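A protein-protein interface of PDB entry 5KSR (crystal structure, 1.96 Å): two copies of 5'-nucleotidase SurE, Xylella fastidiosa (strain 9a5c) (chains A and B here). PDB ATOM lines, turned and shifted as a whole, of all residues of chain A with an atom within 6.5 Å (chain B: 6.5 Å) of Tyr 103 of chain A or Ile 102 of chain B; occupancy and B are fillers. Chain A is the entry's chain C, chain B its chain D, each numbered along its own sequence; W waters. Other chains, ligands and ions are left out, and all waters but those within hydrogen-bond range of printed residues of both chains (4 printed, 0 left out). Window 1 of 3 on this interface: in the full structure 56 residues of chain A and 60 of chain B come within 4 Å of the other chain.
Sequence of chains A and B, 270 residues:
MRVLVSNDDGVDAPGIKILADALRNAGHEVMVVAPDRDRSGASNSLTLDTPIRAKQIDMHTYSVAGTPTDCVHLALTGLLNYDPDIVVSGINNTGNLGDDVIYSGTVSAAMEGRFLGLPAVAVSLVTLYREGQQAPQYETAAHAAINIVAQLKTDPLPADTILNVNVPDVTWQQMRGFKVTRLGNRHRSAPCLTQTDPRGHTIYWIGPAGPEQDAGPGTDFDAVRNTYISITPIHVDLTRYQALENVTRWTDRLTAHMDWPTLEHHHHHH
The backbone NH (N) of His 235 of chain A is in hydrogen-bond range of the backbone carbonyl oxygen (O) of Leu 238 of chain B (3.1 Å).
O of Tyr 103 of chain B sits at hydrogen-bond distance from ND2 of Asn 44 of chain B, at 3.3 Å.
ND2 of Asn 44 of chain A lies within hydrogen-bond range of O of Tyr 103 of chain A.
Ala 42 of chain A touches Ser 43 of chain B (O to CB, 3.5 Å).
O of Ile 102 of chain A touches CE1 of Tyr 103 of chain B (3.8 Å).
Met 111 of chain B touches Ile 102 of chain A.
Leu 238 of chain B touches Ile 102 of chain A.
Ile 102 of chain B touches Tyr 103 of chain A.
OH of Tyr 103 of chain A touches CB of Ser 108 of chain B, 3.2 Å away.
Met 111 of chain A touches Ile 102 of chain B (CE to CD1, 3.6 Å).
Met 111 of chain A touches Tyr 103 of chain B.
Phe 115 of chain A touches Asp 99 of chain B.
Printed residues of chain B within 4 Å of Tyr 103 of chain A: Ile 102 (3.7 Å) and Ser 108 (3.2 Å).
Of the printed residues of chain B, His 235 of chain A touches Leu 238.
Of the printed residues of chain A, Ser 43 of chain B touches Ala 42 (3.5 Å).
Printed residues of chain A within 4 Å of Asp 99 of chain B: Phe 115.
Val 101 of chain B touches none of the printed residues of chain A.
Printed residues of chain A within 4 Å of Ile 102 of chain B: Tyr 103 and Met 111.
Of the printed residues of chain A, Tyr 103 of chain B touches Ile 102 (3.8 Å) and Met 111 (3.99 Å).
Of the printed residues of chain A, Ser 108 of chain B touches Tyr 103 (3.2 Å).
Ala 109 of chain B touches none of the printed residues of chain A.
The nearest printed residue of chain A that does not touch Ile 102 of chain B is Leu 238 of chain A (4.1 Å).
Of the 16 printed residues of chain A, 6 touch a printed residue of chain B.
Hydrophobic or aromatic side chains of chain B within 4 Å of the printed part of chain A: Ile 102, Tyr 103, Met 111 and Leu 238.
Among the printed residues, no Asp or Glu carboxylate lies within 4 Å of a Lys or Arg side-chain nitrogen of the other chain.
Ile 102 of chain A touches Tyr 103 of chain B, and with the chains exchanged Tyr 103 of chain A touches Ile 102 of chain B.
Ile 102 of chain A touches Met 111 of chain B, and with the chains exchanged Met 111 of chain A touches Ile 102 of chain B.
Ile 102 of chain A touches Leu 238 of chain B, but with the chains exchanged Leu 238 of chain A does not touch Ile 102 of chain B (4.1 Å).
Met 111 of chain A touches Tyr 103 of chain B, but with the chains exchanged Tyr 103 of chain A does not touch Met 111 of chain B (4.5 Å).
Of the 10 pairs that touch across the chains among the printed residues, 4 have their exchanged pair printed and touching as well.
Water W3 lies within hydrogen-bond range of OH of Tyr 103 of chain B (2.8 Å), O of Ser 104 of chain A (3.0 Å) and O of Ile 102 of chain A (3.1 Å).
Water W1 lies within hydrogen-bond range of the backbone carbonyl oxygen (O) of Tyr 103 of chain A (2.9 Å) and the side-chain hydroxyl (OG) of Ser 43 of chain B (3.0 Å).
Water W2 lies within hydrogen-bond range of OH of Tyr 103 of chain A (2.9 Å), O of Ile 102 of chain B (3.1 Å) and O of Ser 104 of chain B (3.1 Å).
Water W4 lies within hydrogen-bond range of the side-chain hydroxyl (OG) of Ser 45 of chain B (3.1 Å) and the backbone carbonyl oxygen (O) of Asp 100 of chain A (3.3 Å).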
ATOM      1  N   ALA A  42      -2.947 -23.288 -31.813  1.00  0.00           N
ATOM      2  CA  ALA A  42      -3.064 -24.281 -30.729  1.00  0.00           C
ATOM      3  C   ALA A  42      -3.539 -23.696 -29.366  1.00  0.00           C
ATOM      4  O   ALA A  42      -3.481 -22.478 -29.163  1.00  0.00           O
ATOM      5  CB  ALA A  42      -1.718 -25.021 -30.560  1.00  0.00           C
ATOM      6  N   ASN A  44      -3.469 -22.622 -25.441  1.00  0.00           N
ATOM      7  CA  ASN A  44      -2.391 -22.029 -24.594  1.00  0.00           C
ATOM      8  C   ASN A  44      -2.167 -22.612 -23.169  1.00  0.00           C
ATOM      9  O   ASN A  44      -1.241 -22.149 -22.481  1.00  0.00           O
ATOM     10  CB  ASN A  44      -2.549 -20.496 -24.435  1.00  0.00           C
ATOM     11  CG  ASN A  44      -2.529 -19.726 -25.774  1.00  0.00           C
ATOM     12  OD1 ASN A  44      -1.931 -20.162 -26.746  1.00  0.00           O
ATOM     13  ND2 ASN A  44      -3.206 -18.559 -25.805  1.00  0.00           N
ATOM     14  N   ASP A  99     -10.045  -6.901 -29.205  1.00  0.00           N
ATOM     15  CA  ASP A  99     -10.615  -8.198 -28.812  1.00  0.00           C
ATOM     16  C   ASP A  99      -9.741  -9.418 -29.106  1.00  0.00           C
ATOM     17  O   ASP A  99     -10.100 -10.544 -28.775  1.00  0.00           O
ATOM     18  CB  ASP A  99     -11.978  -8.408 -29.485  1.00  0.00           C
ATOM     19  CG  ASP A  99     -13.102  -7.748 -28.723  1.00  0.00           C
ATOM     20  OD1 ASP A  99     -12.904  -7.514 -27.516  1.00  0.00           O
ATOM     21  OD2 ASP A  99     -14.170  -7.464 -29.324  1.00  0.00           O
ATOM     22  N   ASP A 100      -8.611  -9.218 -29.771  1.00  0.00           N
ATOM     23  CA  ASP A 100      -7.731 -10.343 -30.052  1.00  0.00           C
ATOM     24  C   ASP A 100      -6.807 -10.673 -28.863  1.00  0.00           C
ATOM     25  O   ASP A 100      -6.225 -11.761 -28.812  1.00  0.00           O
ATOM     26  CB  ASP A 100      -6.881 -10.087 -31.298  1.00  0.00           C
ATOM     27  CG  ASP A 100      -7.702 -10.040 -32.591  1.00  0.00           C
ATOM     28  OD1 ASP A 100      -8.869 -10.493 -32.608  1.00  0.00           O
ATOM     29  OD2 ASP A 100      -7.158  -9.546 -33.605  1.00  0.00           O
ATOM     30  N   VAL A 101      -6.658  -9.741 -27.922  1.00  0.00           N
ATOM     31  CA  VAL A 101      -5.657  -9.880 -26.840  1.00  0.00           C
ATOM     32  C   VAL A 101      -5.873 -11.089 -25.868  1.00  0.00           C
ATOM     33  O   VAL A 101      -4.910 -11.798 -25.524  1.00  0.00           O
ATOM     34  CB  VAL A 101      -5.505  -8.518 -26.069  1.00  0.00           C
ATOM     35  CG1 VAL A 101      -4.608  -8.640 -24.830  1.00  0.00           C
ATOM     36  CG2 VAL A 101      -4.954  -7.431 -27.026  1.00  0.00           C
ATOM     37  N   ILE A 102      -7.101 -11.338 -25.408  1.00  0.00           N
ATOM     38  CA  ILE A 102      -7.289 -12.433 -24.408  1.00  0.00           C
ATOM     39  C   ILE A 102      -6.767 -13.827 -24.855  1.00  0.00           C
ATOM     40  O   ILE A 102      -6.202 -14.589 -24.033  1.00  0.00           O
ATOM     41  CB  ILE A 102      -8.762 -12.513 -23.900  1.00  0.00           C
ATOM     42  CG1 ILE A 102      -8.902 -13.581 -22.799  1.00  0.00           C
ATOM     43  CG2 ILE A 102      -9.722 -12.733 -25.078  1.00  0.00           C
ATOM     44  CD1 ILE A 102     -10.185 -13.470 -22.002  1.00  0.00           C
ATOM     45  N   TYR A 103      -6.866 -14.158 -26.139  1.00  0.00           N
ATOM     46  CA  TYR A 103      -6.375 -15.478 -26.594  1.00  0.00           C
ATOM     47  C   TYR A 103      -5.009 -15.499 -27.345  1.00  0.00           C
ATOM     48  O   TYR A 103      -4.672 -16.498 -27.987  1.00  0.00           O
ATOM     49  CB  TYR A 103      -7.476 -16.245 -27.367  1.00  0.00           C
ATOM     50  CG  TYR A 103      -8.761 -16.405 -26.549  1.00  0.00           C
ATOM     51  CD1 TYR A 103      -8.705 -16.837 -25.219  1.00  0.00           C
ATOM     52  CD2 TYR A 103     -10.010 -16.075 -27.077  1.00  0.00           C
ATOM     53  CE1 TYR A 103      -9.870 -16.971 -24.437  1.00  0.00           C
ATOM     54  CE2 TYR A 103     -11.196 -16.187 -26.289  1.00  0.00           C
ATOM     55  CZ  TYR A 103     -11.106 -16.633 -24.969  1.00  0.00           C
ATOM     56  OH  TYR A 103     -12.234 -16.757 -24.154  1.00  0.00           O
ATOM     57  N   SER A 104      -4.245 -14.399 -27.273  1.00  0.00           N
ATOM     58  CA  SER A 104      -2.914 -14.304 -27.930  1.00  0.00           C
ATOM     59  C   SER A 104      -1.814 -15.194 -27.289  1.00  0.00           C
ATOM     60  O   SER A 104      -1.582 -15.102 -26.103  1.00  0.00           O
ATOM     61  CB  SER A 104      -2.428 -12.836 -27.892  1.00  0.00           C
ATOM     62  OG  SER A 104      -1.013 -12.721 -28.106  1.00  0.00           O
ATOM     63  N   GLY A 105      -1.115 -16.012 -28.085  1.00  0.00           N
ATOM     64  CA  GLY A 105      -0.017 -16.832 -27.578  1.00  0.00           C
ATOM     65  C   GLY A 105       1.184 -16.015 -27.087  1.00  0.00           C
ATOM     66  O   GLY A 105       1.828 -16.387 -26.097  1.00  0.00           O
ATOM     67  N   THR A 106       1.474 -14.894 -27.768  1.00  0.00           N
ATOM     68  CA  THR A 106       2.557 -13.979 -27.370  1.00  0.00           C
ATOM     69  C   THR A 106       2.290 -13.399 -25.962  1.00  0.00           C
ATOM     70  O   THR A 106       3.185 -13.407 -25.073  1.00  0.00           O
ATOM     71  CB  THR A 106       2.746 -12.794 -28.386  1.00  0.00           C
ATOM     72  OG1 THR A 106       3.000 -13.294 -29.716  1.00  0.00           O
ATOM     73  CG2 THR A 106       3.927 -11.883 -27.943  1.00  0.00           C
ATOM     74  N   VAL A 107       1.057 -12.920 -25.751  1.00  0.00           N
ATOM     75  CA  VAL A 107       0.598 -12.458 -24.424  1.00  0.00           C
ATOM     76  C   VAL A 107       0.669 -13.550 -23.308  1.00  0.00           C
ATOM     77  O   VAL A 107       1.030 -13.240 -22.162  1.00  0.00           O
ATOM     78  CB  VAL A 107      -0.830 -11.801 -24.513  1.00  0.00           C
ATOM     79  CG1 VAL A 107      -1.378 -11.431 -23.121  1.00  0.00           C
ATOM     80  CG2 VAL A 107      -0.792 -10.546 -25.464  1.00  0.00           C
ATOM     81  N   MET A 111       2.188 -13.419 -19.237  1.00  0.00           N
ATOM     82  CA  MET A 111       1.320 -13.707 -18.082  1.00  0.00           C
ATOM     83  C   MET A 111       1.917 -14.728 -17.072  1.00  0.00           C
ATOM     84  O   MET A 111       1.857 -14.508 -15.838  1.00  0.00           O
ATOM     85  CB  MET A 111      -0.055 -14.181 -18.556  1.00  0.00           C
ATOM     86  CG  MET A 111      -1.155 -13.969 -17.516  1.00  0.00           C
ATOM     87  SD  MET A 111      -2.290 -12.652 -17.993  1.00  0.00           S
ATOM     88  CE  MET A 111      -2.862 -13.276 -19.566  1.00  0.00           C
ATOM     89  N   PHE A 115       2.830 -14.269 -12.873  1.00  0.00           N
ATOM     90  CA  PHE A 115       2.304 -15.284 -11.946  1.00  0.00           C
ATOM     91  C   PHE A 115       3.387 -15.871 -11.027  1.00  0.00           C
ATOM     92  O   PHE A 115       3.134 -16.138  -9.848  1.00  0.00           O
ATOM     93  CB  PHE A 115       1.638 -16.444 -12.709  1.00  0.00           C
ATOM     94  CG  PHE A 115       0.252 -16.140 -13.228  1.00  0.00           C
ATOM     95  CD1 PHE A 115      -0.389 -14.945 -12.918  1.00  0.00           C
ATOM     96  CD2 PHE A 115      -0.409 -17.060 -14.023  1.00  0.00           C
ATOM     97  CE1 PHE A 115      -1.673 -14.677 -13.394  1.00  0.00           C
ATOM     98  CE2 PHE A 115      -1.688 -16.808 -14.499  1.00  0.00           C
ATOM     99  CZ  PHE A 115      -2.328 -15.611 -14.186  1.00  0.00           C
ATOM    100  N   HIS A 235      -4.985  -6.349 -16.879  1.00  0.00           N
ATOM    101  CA  HIS A 235      -5.135  -7.149 -15.631  1.00  0.00           C
ATOM    102  C   HIS A 235      -4.426  -8.504 -15.708  1.00  0.00           C
ATOM    103  O   HIS A 235      -4.409  -9.126 -16.765  1.00  0.00           O
ATOM    104  CB  HIS A 235      -6.623  -7.515 -15.365  1.00  0.00           C
ATOM    105  CG  HIS A 235      -7.519  -6.372 -14.970  1.00  0.00           C
ATOM    106  ND1 HIS A 235      -7.459  -5.764 -13.734  1.00  0.00           N
ATOM    107  CD2 HIS A 235      -8.556  -5.783 -15.626  1.00  0.00           C
ATOM    108  CE1 HIS A 235      -8.401  -4.833 -13.651  1.00  0.00           C
ATOM    109  NE2 HIS A 235      -9.079  -4.827 -14.786  1.00  0.00           N
ATOM    110  N   VAL A 236      -3.886  -8.994 -14.589  1.00  0.00           N
ATOM    111  CA  VAL A 236      -3.513 -10.410 -14.499  1.00  0.00           C
ATOM    112  C   VAL A 236      -4.451 -11.326 -13.629  1.00  0.00           C
ATOM    113  O   VAL A 236      -4.346 -12.539 -13.726  1.00  0.00           O
ATOM    114  CB  VAL A 236      -2.032 -10.603 -14.077  1.00  0.00           C
ATOM    115  CG1 VAL A 236      -1.093  -9.831 -15.028  1.00  0.00           C
ATOM    116  CG2 VAL A 236      -1.820 -10.162 -12.648  1.00  0.00           C
ATOM    117  N   LEU A 238      -8.473 -12.184 -13.038  1.00  0.00           N
ATOM    118  CA  LEU A 238      -9.808 -11.957 -13.631  1.00  0.00           C
ATOM    119  C   LEU A 238     -10.960 -11.789 -12.614  1.00  0.00           C
ATOM    120  O   LEU A 238     -12.120 -11.558 -13.006  1.00  0.00           O
ATOM    121  CB  LEU A 238     -10.161 -13.056 -14.646  1.00  0.00           C
ATOM    122  CG  LEU A 238      -9.729 -12.882 -16.114  1.00  0.00           C
ATOM    123  CD1 LEU A 238      -8.214 -12.978 -16.262  1.00  0.00           C
ATOM    124  CD2 LEU A 238     -10.426 -13.890 -17.029  1.00  0.00           C
ATOM    125  N   SER B  43      -7.502 -24.214 -29.769  1.00  0.00           N
ATOM    126  CA  SER B  43      -7.487 -22.755 -29.540  1.00  0.00           C
ATOM    127  C   SER B  43      -8.905 -22.157 -29.570  1.00  0.00           C
ATOM    128  O   SER B  43      -9.737 -22.619 -30.364  1.00  0.00           O
ATOM    129  CB  SER B  43      -6.626 -22.080 -30.628  1.00  0.00           C
ATOM    130  OG  SER B  43      -6.911 -20.687 -30.792  1.00  0.00           O
ATOM    131  N   ASN B  44      -9.166 -21.134 -28.742  1.00  0.00           N
ATOM    132  CA  ASN B  44     -10.524 -20.520 -28.624  1.00  0.00           C
ATOM    133  C   ASN B  44     -10.872 -19.314 -29.574  1.00  0.00           C
ATOM    134  O   ASN B  44     -12.006 -18.826 -29.539  1.00  0.00           O
ATOM    135  CB  ASN B  44     -10.857 -20.111 -27.148  1.00  0.00           C
ATOM    136  CG  ASN B  44     -10.769 -21.289 -26.134  1.00  0.00           C
ATOM    137  OD1 ASN B  44     -10.966 -22.441 -26.479  1.00  0.00           O
ATOM    138  ND2 ASN B  44     -10.495 -20.967 -24.869  1.00  0.00           N
ATOM    139  N   SER B  45      -9.943 -18.850 -30.423  1.00  0.00           N
ATOM    140  CA  SER B  45     -10.174 -17.657 -31.295  1.00  0.00           C
ATOM    141  C   SER B  45     -11.369 -17.774 -32.304  1.00  0.00           C
ATOM    142  O   SER B  45     -11.762 -18.883 -32.673  1.00  0.00           O
ATOM    143  CB  SER B  45      -8.906 -17.348 -32.111  1.00  0.00           C
ATOM    144  OG  SER B  45      -7.782 -16.992 -31.299  1.00  0.00           O
ATOM    145  N   LEU B  46     -11.914 -16.639 -32.757  1.00  0.00           N
ATOM    146  CA  LEU B  46     -12.882 -16.617 -33.887  1.00  0.00           C
ATOM    147  C   LEU B  46     -12.199 -17.000 -35.220  1.00  0.00           C
ATOM    148  O   LEU B  46     -11.039 -16.597 -35.470  1.00  0.00           O
ATOM    149  CB  LEU B  46     -13.525 -15.233 -34.040  1.00  0.00           C
ATOM    150  CG  LEU B  46     -14.566 -14.674 -33.061  1.00  0.00           C
ATOM    151  CD1 LEU B  46     -14.852 -13.208 -33.385  1.00  0.00           C
ATOM    152  CD2 LEU B  46     -15.892 -15.474 -33.092  1.00  0.00           C
ATOM    153  N   THR B  69     -16.732 -20.122 -29.560  1.00  0.00           N
ATOM    154  CA  THR B  69     -16.996 -18.731 -29.965  1.00  0.00           C
ATOM    155  C   THR B  69     -17.656 -18.583 -31.353  1.00  0.00           C
ATOM    156  O   THR B  69     -18.489 -17.680 -31.520  1.00  0.00           O
ATOM    157  CB  THR B  69     -15.757 -17.777 -29.887  1.00  0.00           C
ATOM    158  OG1 THR B  69     -14.740 -18.264 -30.765  1.00  0.00           O
ATOM    159  CG2 THR B  69     -15.202 -17.712 -28.461  1.00  0.00           C
ATOM    160  N   GLY B  98      -9.778 -21.575 -10.366  1.00  0.00           N
ATOM    161  CA  GLY B  98      -8.504 -20.860 -10.212  1.00  0.00           C
ATOM    162  C   GLY B  98      -7.760 -20.471 -11.496  1.00  0.00           C
ATOM    163  O   GLY B  98      -8.318 -19.761 -12.341  1.00  0.00           O
ATOM    164  N   ASP B  99      -6.509 -20.920 -11.642  1.00  0.00           N
ATOM    165  CA  ASP B  99      -5.685 -20.601 -12.824  1.00  0.00           C
ATOM    166  C   ASP B  99      -6.140 -21.250 -14.132  1.00  0.00           C
ATOM    167  O   ASP B  99      -5.556 -21.005 -15.190  1.00  0.00           O
ATOM    168  CB  ASP B  99      -4.214 -20.975 -12.582  1.00  0.00           C
ATOM    169  CG  ASP B  99      -3.433 -19.863 -11.913  1.00  0.00           C
ATOM    170  OD1 ASP B  99      -3.847 -18.699 -12.057  1.00  0.00           O
ATOM    171  OD2 ASP B  99      -2.411 -20.150 -11.249  1.00  0.00           O
ATOM    172  N   ASP B 100      -7.151 -22.105 -14.066  1.00  0.00           N
ATOM    173  CA  ASP B 100      -7.656 -22.739 -15.277  1.00  0.00           C
ATOM    174  C   ASP B 100      -8.664 -21.835 -16.038  1.00  0.00           C
ATOM    175  O   ASP B 100      -8.937 -22.064 -17.218  1.00  0.00           O
ATOM    176  CB  ASP B 100      -8.255 -24.126 -14.972  1.00  0.00           C
ATOM    177  CG  ASP B 100      -7.214 -25.123 -14.417  1.00  0.00           C
ATOM    178  OD1 ASP B 100      -5.991 -24.880 -14.540  1.00  0.00           O
ATOM    179  OD2 ASP B 100      -7.626 -26.163 -13.854  1.00  0.00           O
ATOM    180  N   VAL B 101      -9.184 -20.796 -15.385  1.00  0.00           N
ATOM    181  CA  VAL B 101     -10.293 -20.005 -15.970  1.00  0.00           C
ATOM    182  C   VAL B 101      -9.989 -19.215 -17.292  1.00  0.00           C
ATOM    183  O   VAL B 101     -10.781 -19.273 -18.258  1.00  0.00           O
ATOM    184  CB  VAL B 101     -10.981 -19.122 -14.871  1.00  0.00           C
ATOM    185  CG1 VAL B 101     -12.043 -18.212 -15.434  1.00  0.00           C
ATOM    186  CG2 VAL B 101     -11.583 -20.029 -13.764  1.00  0.00           C
ATOM    187  N   ILE B 102      -8.872 -18.490 -17.364  1.00  0.00           N
ATOM    188  CA  ILE B 102      -8.632 -17.661 -18.572  1.00  0.00           C
ATOM    189  C   ILE B 102      -8.587 -18.483 -19.882  1.00  0.00           C
ATOM    190  O   ILE B 102      -9.023 -18.000 -20.944  1.00  0.00           O
ATOM    191  CB  ILE B 102      -7.369 -16.747 -18.425  1.00  0.00           C
ATOM    192  CG1 ILE B 102      -7.168 -15.863 -19.674  1.00  0.00           C
ATOM    193  CG2 ILE B 102      -6.127 -17.589 -18.104  1.00  0.00           C
ATOM    194  CD1 ILE B 102      -6.214 -14.683 -19.433  1.00  0.00           C
ATOM    195  N   TYR B 103      -8.143 -19.743 -19.836  1.00  0.00           N
ATOM    196  CA  TYR B 103      -8.108 -20.506 -21.098  1.00  0.00           C
ATOM    197  C   TYR B 103      -9.213 -21.600 -21.322  1.00  0.00           C
ATOM    198  O   TYR B 103      -9.108 -22.394 -22.254  1.00  0.00           O
ATOM    199  CB  TYR B 103      -6.678 -21.024 -21.395  1.00  0.00           C
ATOM    200  CG  TYR B 103      -5.633 -19.890 -21.469  1.00  0.00           C
ATOM    201  CD1 TYR B 103      -5.896 -18.725 -22.197  1.00  0.00           C
ATOM    202  CD2 TYR B 103      -4.423 -19.969 -20.779  1.00  0.00           C
ATOM    203  CE1 TYR B 103      -4.980 -17.666 -22.245  1.00  0.00           C
ATOM    204  CE2 TYR B 103      -3.475 -18.903 -20.830  1.00  0.00           C
ATOM    205  CZ  TYR B 103      -3.769 -17.761 -21.570  1.00  0.00           C
ATOM    206  OH  TYR B 103      -2.878 -16.691 -21.629  1.00  0.00           O
ATOM    207  N   SER B 104     -10.274 -21.593 -20.500  1.00  0.00           N
ATOM    208  CA  SER B 104     -11.389 -22.568 -20.579  1.00  0.00           C
ATOM    209  C   SER B 104     -12.318 -22.392 -21.817  1.00  0.00           C
ATOM    210  O   SER B 104     -12.826 -21.297 -22.052  1.00  0.00           O
ATOM    211  CB  SER B 104     -12.244 -22.445 -19.302  1.00  0.00           C
ATOM    212  OG  SER B 104     -13.512 -23.097 -19.436  1.00  0.00           O
ATOM    213  N   VAL B 107     -15.956 -21.353 -20.647  1.00  0.00           N
ATOM    214  CA  VAL B 107     -16.000 -19.897 -20.361  1.00  0.00           C
ATOM    215  C   VAL B 107     -16.034 -19.020 -21.650  1.00  0.00           C
ATOM    216  O   VAL B 107     -16.736 -17.991 -21.684  1.00  0.00           O
ATOM    217  CB  VAL B 107     -14.854 -19.451 -19.342  1.00  0.00           C
ATOM    218  CG1 VAL B 107     -14.753 -17.925 -19.194  1.00  0.00           C
ATOM    219  CG2 VAL B 107     -15.047 -20.126 -17.954  1.00  0.00           C
ATOM    220  N   SER B 108     -15.300 -19.413 -22.706  1.00  0.00           N
ATOM    221  CA  SER B 108     -15.252 -18.592 -23.951  1.00  0.00           C
ATOM    222  C   SER B 108     -16.618 -18.381 -24.622  1.00  0.00           C
ATOM    223  O   SER B 108     -16.859 -17.327 -25.244  1.00  0.00           O
ATOM    224  CB  SER B 108     -14.221 -19.129 -24.990  1.00  0.00           C
ATOM    225  OG  SER B 108     -14.634 -20.371 -25.588  1.00  0.00           O
ATOM    226  N   ALA B 109     -17.515 -19.367 -24.550  1.00  0.00           N
ATOM    227  CA  ALA B 109     -18.852 -19.162 -25.186  1.00  0.00           C
ATOM    228  C   ALA B 109     -19.728 -18.140 -24.431  1.00  0.00           C
ATOM    229  O   ALA B 109     -20.500 -17.367 -25.054  1.00  0.00           O
ATOM    230  CB  ALA B 109     -19.591 -20.505 -25.340  1.00  0.00           C
ATOM    231  N   MET B 111     -18.477 -15.559 -22.681  1.00  0.00           N
ATOM    232  CA  MET B 111     -17.844 -14.274 -23.024  1.00  0.00           C
ATOM    233  C   MET B 111     -18.418 -13.635 -24.316  1.00  0.00           C
ATOM    234  O   MET B 111     -18.787 -12.443 -24.322  1.00  0.00           O
ATOM    235  CB  MET B 111     -16.325 -14.471 -23.142  1.00  0.00           C
ATOM    236  CG  MET B 111     -15.515 -13.169 -23.129  1.00  0.00           C
ATOM    237  SD  MET B 111     -15.026 -12.626 -21.474  1.00  0.00           S
ATOM    238  CE  MET B 111     -13.847 -13.889 -21.015  1.00  0.00           C
ATOM    239  N   LEU B 238     -10.341  -6.497 -20.363  1.00  0.00           N
ATOM    240  CA  LEU B 238      -8.975  -6.644 -19.795  1.00  0.00           C
ATOM    241  C   LEU B 238      -8.211  -5.322 -19.552  1.00  0.00           C
ATOM    242  O   LEU B 238      -7.118  -5.337 -18.951  1.00  0.00           O
ATOM    243  CB  LEU B 238      -8.105  -7.620 -20.631  1.00  0.00           C
ATOM    244  CG  LEU B 238      -8.207  -9.152 -20.466  1.00  0.00           C
ATOM    245  CD1 LEU B 238      -7.186  -9.918 -21.351  1.00  0.00           C
ATOM    246  CD2 LEU B 238      -8.079  -9.610 -19.005  1.00  0.00           C
HETATM  247  O   HOH W   1      -4.945 -19.073 -29.219  1.00  0.00           O
HETATM  248  O   HOH W   2     -12.021 -18.306 -21.662  1.00  0.00           O
HETATM  249  O   HOH W   3      -3.179 -14.727 -23.579  1.00  0.00           O
HETATM  250  O   HOH W   4      -7.565 -13.937 -30.835  1.00  0.00           O
